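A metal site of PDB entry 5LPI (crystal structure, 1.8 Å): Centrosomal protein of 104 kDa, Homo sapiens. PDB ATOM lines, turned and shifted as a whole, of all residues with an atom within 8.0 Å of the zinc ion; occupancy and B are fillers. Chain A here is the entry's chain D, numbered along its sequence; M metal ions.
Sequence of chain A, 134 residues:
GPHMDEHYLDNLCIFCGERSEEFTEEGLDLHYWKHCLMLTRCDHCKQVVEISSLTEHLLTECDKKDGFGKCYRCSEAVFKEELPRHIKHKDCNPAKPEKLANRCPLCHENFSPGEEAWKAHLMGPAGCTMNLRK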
ATOM      1  N   ARG A  41     -12.879  14.615 -23.701  1.00  0.00           N
ATOM      2  CA  ARG A  41     -11.607  14.406 -24.385  1.00  0.00           C
ATOM      3  C   ARG A  41     -11.383  15.552 -25.358  1.00  0.00           C
ATOM      4  O   ARG A  41     -12.197  15.778 -26.246  1.00  0.00           O
ATOM      5  CB  ARG A  41     -11.596  13.106 -25.181  1.00  0.00           C
ATOM      6  CG  ARG A  41     -11.263  11.878 -24.434  1.00  0.00           C
ATOM      7  CD  ARG A  41     -11.315  10.677 -25.390  1.00  0.00           C
ATOM      8  NE  ARG A  41     -11.942   9.550 -24.729  1.00  0.00           N
ATOM      9  CZ  ARG A  41     -12.399   8.483 -25.359  1.00  0.00           C
ATOM     10  NH1 ARG A  41     -12.309   8.384 -26.680  1.00  0.00           N
ATOM     11  NH2 ARG A  41     -12.952   7.515 -24.652  1.00  0.00           N
ATOM     12  N   CYS A  42     -10.245  16.233 -25.237  1.00  0.00           N
ATOM     13  CA  CYS A  42      -9.936  17.263 -26.221  1.00  0.00           C
ATOM     14  C   CYS A  42      -9.737  16.626 -27.592  1.00  0.00           C
ATOM     15  O   CYS A  42      -8.876  15.751 -27.759  1.00  0.00           O
ATOM     16  CB  CYS A  42      -8.681  18.033 -25.813  1.00  0.00           C
ATOM     17  SG  CYS A  42      -8.274  19.290 -27.023  1.00  0.00           S
ATOM     18  N   ASP A  43     -10.517  17.048 -28.591  1.00  0.00           N
ATOM     19  CA  ASP A  43     -10.373  16.424 -29.903  1.00  0.00           C
ATOM     20  C   ASP A  43      -9.035  16.786 -30.546  1.00  0.00           C
ATOM     21  O   ASP A  43      -8.561  16.049 -31.430  1.00  0.00           O
ATOM     22  CB  ASP A  43     -11.525  16.842 -30.825  1.00  0.00           C
ATOM     23  CG  ASP A  43     -11.633  15.970 -32.083  1.00  0.00           C
ATOM     24  OD1 ASP A  43     -11.138  14.815 -32.083  1.00  0.00           O
ATOM     25  OD2 ASP A  43     -12.234  16.434 -33.070  1.00  0.00           O
ATOM     26  N   HIS A  44      -8.391  17.870 -30.111  1.00  0.00           N
ATOM     27  CA  HIS A  44      -7.185  18.338 -30.773  1.00  0.00           C
ATOM     28  C   HIS A  44      -5.926  17.633 -30.268  1.00  0.00           C
ATOM     29  O   HIS A  44      -5.048  17.311 -31.068  1.00  0.00           O
ATOM     30  CB  HIS A  44      -7.106  19.858 -30.604  1.00  0.00           C
ATOM     31  CG  HIS A  44      -8.375  20.537 -31.004  1.00  0.00           C
ATOM     32  ND1 HIS A  44      -8.764  20.664 -32.318  1.00  0.00           N
ATOM     33  CD2 HIS A  44      -9.406  21.033 -30.263  1.00  0.00           C
ATOM     34  CE1 HIS A  44      -9.942  21.267 -32.376  1.00  0.00           C
ATOM     35  NE2 HIS A  44     -10.357  21.482 -31.139  1.00  0.00           N
ATOM     36  N   CYS A  45      -5.844  17.346 -28.955  1.00  0.00           N
ATOM     37  CA  CYS A  45      -4.675  16.735 -28.364  1.00  0.00           C
ATOM     38  C   CYS A  45      -4.943  15.364 -27.762  1.00  0.00           C
ATOM     39  O   CYS A  45      -3.992  14.681 -27.369  1.00  0.00           O
ATOM     40  CB  CYS A  45      -4.092  17.651 -27.276  1.00  0.00           C
ATOM     41  SG  CYS A  45      -5.062  17.689 -25.770  1.00  0.00           S
ATOM     42  N   LYS A  46      -6.208  14.943 -27.689  1.00  0.00           N
ATOM     43  CA  LYS A  46      -6.687  13.660 -27.172  1.00  0.00           C
ATOM     44  C   LYS A  46      -6.497  13.495 -25.665  1.00  0.00           C
ATOM     45  O   LYS A  46      -6.633  12.372 -25.146  1.00  0.00           O
ATOM     46  CB  LYS A  46      -6.054  12.458 -27.905  1.00  0.00           C
ATOM     47  CG  LYS A  46      -6.001  12.619 -29.428  1.00  0.00           C
ATOM     48  CD  LYS A  46      -7.350  12.886 -30.077  1.00  0.00           C
ATOM     49  CE  LYS A  46      -7.198  13.017 -31.600  1.00  0.00           C
ATOM     50  NZ  LYS A  46      -8.518  13.205 -32.262  1.00  0.00           N
ATOM     51  N   GLN A  47      -6.217  14.567 -24.932  1.00  0.00           N
ATOM     52  CA  GLN A  47      -6.163  14.520 -23.477  1.00  0.00           C
ATOM     53  C   GLN A  47      -7.559  14.720 -22.904  1.00  0.00           C
ATOM     54  O   GLN A  47      -8.404  15.377 -23.507  1.00  0.00           O
ATOM     55  CB  GLN A  47      -5.247  15.611 -22.934  1.00  0.00           C
ATOM     56  CG  GLN A  47      -3.815  15.478 -23.382  1.00  0.00           C
ATOM     57  CD  GLN A  47      -3.050  14.488 -22.554  1.00  0.00           C
ATOM     58  OE1 GLN A  47      -2.727  13.399 -23.021  1.00  0.00           O
ATOM     59  NE2 GLN A  47      -2.771  14.839 -21.303  1.00  0.00           N
ATOM     60  N   VAL A  48      -7.787  14.170 -21.702  1.00  0.00           N
ATOM     61  CA  VAL A  48      -9.010  14.442 -20.947  1.00  0.00           C
ATOM     62  C   VAL A  48      -8.855  15.789 -20.239  1.00  0.00           C
ATOM     63  O   VAL A  48      -7.844  16.045 -19.580  1.00  0.00           O
ATOM     64  CB  VAL A  48      -9.310  13.329 -19.939  1.00  0.00           C
ATOM     65  CG1 VAL A  48     -10.636  13.615 -19.190  1.00  0.00           C
ATOM     66  CG2 VAL A  48      -9.407  11.982 -20.637  1.00  0.00           C
ATOM     67  N   VAL A  49      -9.886  16.635 -20.342  1.00  0.00           N
ATOM     68  CA  VAL A  49      -9.863  17.937 -19.675  1.00  0.00           C
ATOM     69  C   VAL A  49     -11.221  18.195 -19.011  1.00  0.00           C
ATOM     70  O   VAL A  49     -12.254  17.662 -19.441  1.00  0.00           O
ATOM     71  CB  VAL A  49      -9.523  19.096 -20.653  1.00  0.00           C
ATOM     72  CG1 VAL A  49      -8.214  18.832 -21.393  1.00  0.00           C
ATOM     73  CG2 VAL A  49     -10.641  19.318 -21.618  1.00  0.00           C
ATOM     74  N   LEU A  54     -12.095  24.032 -20.282  1.00  0.00           N
ATOM     75  CA  LEU A  54     -11.744  23.663 -21.655  1.00  0.00           C
ATOM     76  C   LEU A  54     -11.205  24.852 -22.431  1.00  0.00           C
ATOM     77  O   LEU A  54     -10.208  24.721 -23.145  1.00  0.00           O
ATOM     78  CB  LEU A  54     -12.958  23.057 -22.367  1.00  0.00           C
ATOM     79  CG  LEU A  54     -12.788  22.730 -23.853  1.00  0.00           C
ATOM     80  CD1 LEU A  54     -11.687  21.703 -24.104  1.00  0.00           C
ATOM     81  CD2 LEU A  54     -14.108  22.262 -24.459  1.00  0.00           C
ATOM     82  N   HIS A  57      -7.795  25.468 -21.288  1.00  0.00           N
ATOM     83  CA  HIS A  57      -6.949  24.409 -21.838  1.00  0.00           C
ATOM     84  C   HIS A  57      -6.546  24.724 -23.266  1.00  0.00           C
ATOM     85  O   HIS A  57      -5.354  24.710 -23.614  1.00  0.00           O
ATOM     86  CB  HIS A  57      -7.670  23.057 -21.792  1.00  0.00           C
ATOM     87  CG  HIS A  57      -7.025  22.001 -22.652  1.00  0.00           C
ATOM     88  ND1 HIS A  57      -5.954  21.248 -22.224  1.00  0.00           N
ATOM     89  CD2 HIS A  57      -7.286  21.605 -23.922  1.00  0.00           C
ATOM     90  CE1 HIS A  57      -5.593  20.419 -23.194  1.00  0.00           C
ATOM     91  NE2 HIS A  57      -6.385  20.617 -24.226  1.00  0.00           N
ATOM     92  N   LEU A  58      -7.534  24.998 -24.116  1.00  0.00           N
ATOM     93  CA  LEU A  58      -7.265  25.216 -25.532  1.00  0.00           C
ATOM     94  C   LEU A  58      -6.331  26.394 -25.752  1.00  0.00           C
ATOM     95  O   LEU A  58      -5.499  26.381 -26.667  1.00  0.00           O
ATOM     96  CB  LEU A  58      -8.587  25.430 -26.290  1.00  0.00           C
ATOM     97  CG  LEU A  58      -9.522  24.218 -26.368  1.00  0.00           C
ATOM     98  CD1 LEU A  58     -10.898  24.669 -26.870  1.00  0.00           C
ATOM     99  CD2 LEU A  58      -8.934  23.094 -27.269  1.00  0.00           C
ATOM    100  N   LEU A  59      -6.449  27.429 -24.910  1.00  0.00           N
ATOM    101  CA  LEU A  59      -5.664  28.643 -25.142  1.00  0.00           C
ATOM    102  C   LEU A  59      -4.278  28.607 -24.525  1.00  0.00           C
ATOM    103  O   LEU A  59      -3.352  29.231 -25.064  1.00  0.00           O
ATOM    104  CB  LEU A  59      -6.422  29.856 -24.604  1.00  0.00           C
ATOM    105  CG  LEU A  59      -7.739  30.203 -25.316  1.00  0.00           C
ATOM    106  CD1 LEU A  59      -8.476  31.306 -24.578  1.00  0.00           C
ATOM    107  CD2 LEU A  59      -7.451  30.603 -26.749  1.00  0.00           C
ATOM    108  N   GLU A  61      -2.760  25.540 -22.710  1.00  0.00           N
ATOM    109  CA  GLU A  61      -2.179  24.283 -22.255  1.00  0.00           C
ATOM    110  C   GLU A  61      -2.092  23.225 -23.349  1.00  0.00           C
ATOM    111  O   GLU A  61      -1.094  22.492 -23.414  1.00  0.00           O
ATOM    112  CB  GLU A  61      -3.012  23.757 -21.090  1.00  0.00           C
ATOM    113  CG  GLU A  61      -2.546  22.449 -20.507  1.00  0.00           C
ATOM    114  CD  GLU A  61      -3.402  22.031 -19.324  1.00  0.00           C
ATOM    115  OE1 GLU A  61      -4.458  22.657 -19.116  1.00  0.00           O
ATOM    116  OE2 GLU A  61      -3.013  21.082 -18.624  1.00  0.00           O
ATOM    117  N   CYS A  62      -3.117  23.122 -24.203  1.00  0.00           N
ATOM    118  CA  CYS A  62      -3.200  22.107 -25.238  1.00  0.00           C
ATOM    119  C   CYS A  62      -1.931  22.060 -26.089  1.00  0.00           C
ATOM    120  O   CYS A  62      -1.324  23.085 -26.393  1.00  0.00           O
ATOM    121  CB  CYS A  62      -4.406  22.429 -26.129  1.00  0.00           C
ATOM    122  SG  CYS A  62      -4.846  21.221 -27.369  1.00  0.00           S
ATOM    123  N   ASP A  63      -1.548  20.828 -26.488  1.00  0.00           N
ATOM    124  CA  ASP A  63      -0.511  20.662 -27.513  1.00  0.00           C
ATOM    125  C   ASP A  63      -0.783  21.535 -28.726  1.00  0.00           C
ATOM    126  O   ASP A  63       0.170  21.969 -29.398  1.00  0.00           O
ATOM    127  CB  ASP A  63      -0.432  19.212 -27.994  1.00  0.00           C
ATOM    128  CG  ASP A  63       0.117  18.272 -26.933  1.00  0.00           C
ATOM    129  OD1 ASP A  63       0.824  18.731 -26.021  1.00  0.00           O
ATOM    130  OD2 ASP A  63      -0.165  17.059 -27.030  1.00  0.00           O
ATOM    131  N   LYS A  64      -2.051  21.780 -29.054  1.00  0.00           N
ATOM    132  CA  LYS A  64      -2.417  22.543 -30.245  1.00  0.00           C
ATOM    133  C   LYS A  64      -2.748  24.013 -29.959  1.00  0.00           C
ATOM    134  O   LYS A  64      -3.318  24.687 -30.817  1.00  0.00           O
ATOM    135  CB  LYS A  64      -3.596  21.872 -30.962  1.00  0.00           C
ATOM    136  CG  LYS A  64      -3.399  20.347 -31.239  1.00  0.00           C
ATOM    137  CD  LYS A  64      -2.122  20.056 -32.039  1.00  0.00           C
ATOM    138  CE  LYS A  64      -1.928  18.554 -32.220  1.00  0.00           C
ATOM    139  NZ  LYS A  64      -0.654  18.234 -32.955  1.00  0.00           N
ATOM    140  N   LYS A  65      -2.368  24.528 -28.777  1.00  0.00           N
ATOM    141  CA  LYS A  65      -2.815  25.862 -28.357  1.00  0.00           C
ATOM    142  C   LYS A  65      -2.379  26.965 -29.310  1.00  0.00           C
ATOM    143  O   LYS A  65      -3.072  27.990 -29.433  1.00  0.00           O
ATOM    144  CB  LYS A  65      -2.306  26.176 -26.943  1.00  0.00           C
ATOM    145  CG  LYS A  65      -0.810  26.451 -26.879  1.00  0.00           C
ATOM    146  CD  LYS A  65      -0.339  26.478 -25.428  1.00  0.00           C
ATOM    147  CE  LYS A  65       1.087  27.014 -25.316  1.00  0.00           C
ATOM    148  NZ  LYS A  65       1.489  27.067 -23.895  1.00  0.00           N
ATOM    149  N   PHE A  68      -5.003  28.316 -31.778  1.00  0.00           N
ATOM    150  CA  PHE A  68      -6.224  28.966 -31.309  1.00  0.00           C
ATOM    151  C   PHE A  68      -5.949  30.402 -30.866  1.00  0.00           C
ATOM    152  O   PHE A  68      -4.861  30.732 -30.396  1.00  0.00           O
ATOM    153  CB  PHE A  68      -6.846  28.220 -30.120  1.00  0.00           C
ATOM    154  CG  PHE A  68      -7.293  26.837 -30.467  1.00  0.00           C
ATOM    155  CD1 PHE A  68      -8.401  26.640 -31.282  1.00  0.00           C
ATOM    156  CD2 PHE A  68      -6.613  25.730 -29.993  1.00  0.00           C
ATOM    157  CE1 PHE A  68      -8.824  25.336 -31.615  1.00  0.00           C
ATOM    158  CE2 PHE A  68      -7.037  24.443 -30.302  1.00  0.00           C
ATOM    159  CZ  PHE A  68      -8.133  24.244 -31.125  1.00  0.00           C
HETATM  160 ZN    ZN M   1      -6.180  19.778 -26.111  1.00  0.00          ZN
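The backbone NH (N) of Cys 42 is in hydrogen-bond range of the backbone carbonyl oxygen (O) of Gln 47.
N of Gln 47 sits close to SG of Cys 45, 3.4 Å away.
SG of Cys 42 sits close to N of His 44, at 3.4 Å.
The backbone NH (N) of Lys 64 lies close to the side-chain sulfur (SG) of Cys 62 (3.3 Å).
Four residues have an atom within 4 Å of the zinc ion: Cys 42, Cys 45, His 57 and Cys 62.
The zinc ion is bound by NE2 of His 57, SG of Cys 62, SG of Cys 42 and SG of Cys 45.
The zinc ion has four donor atoms within binding distance.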
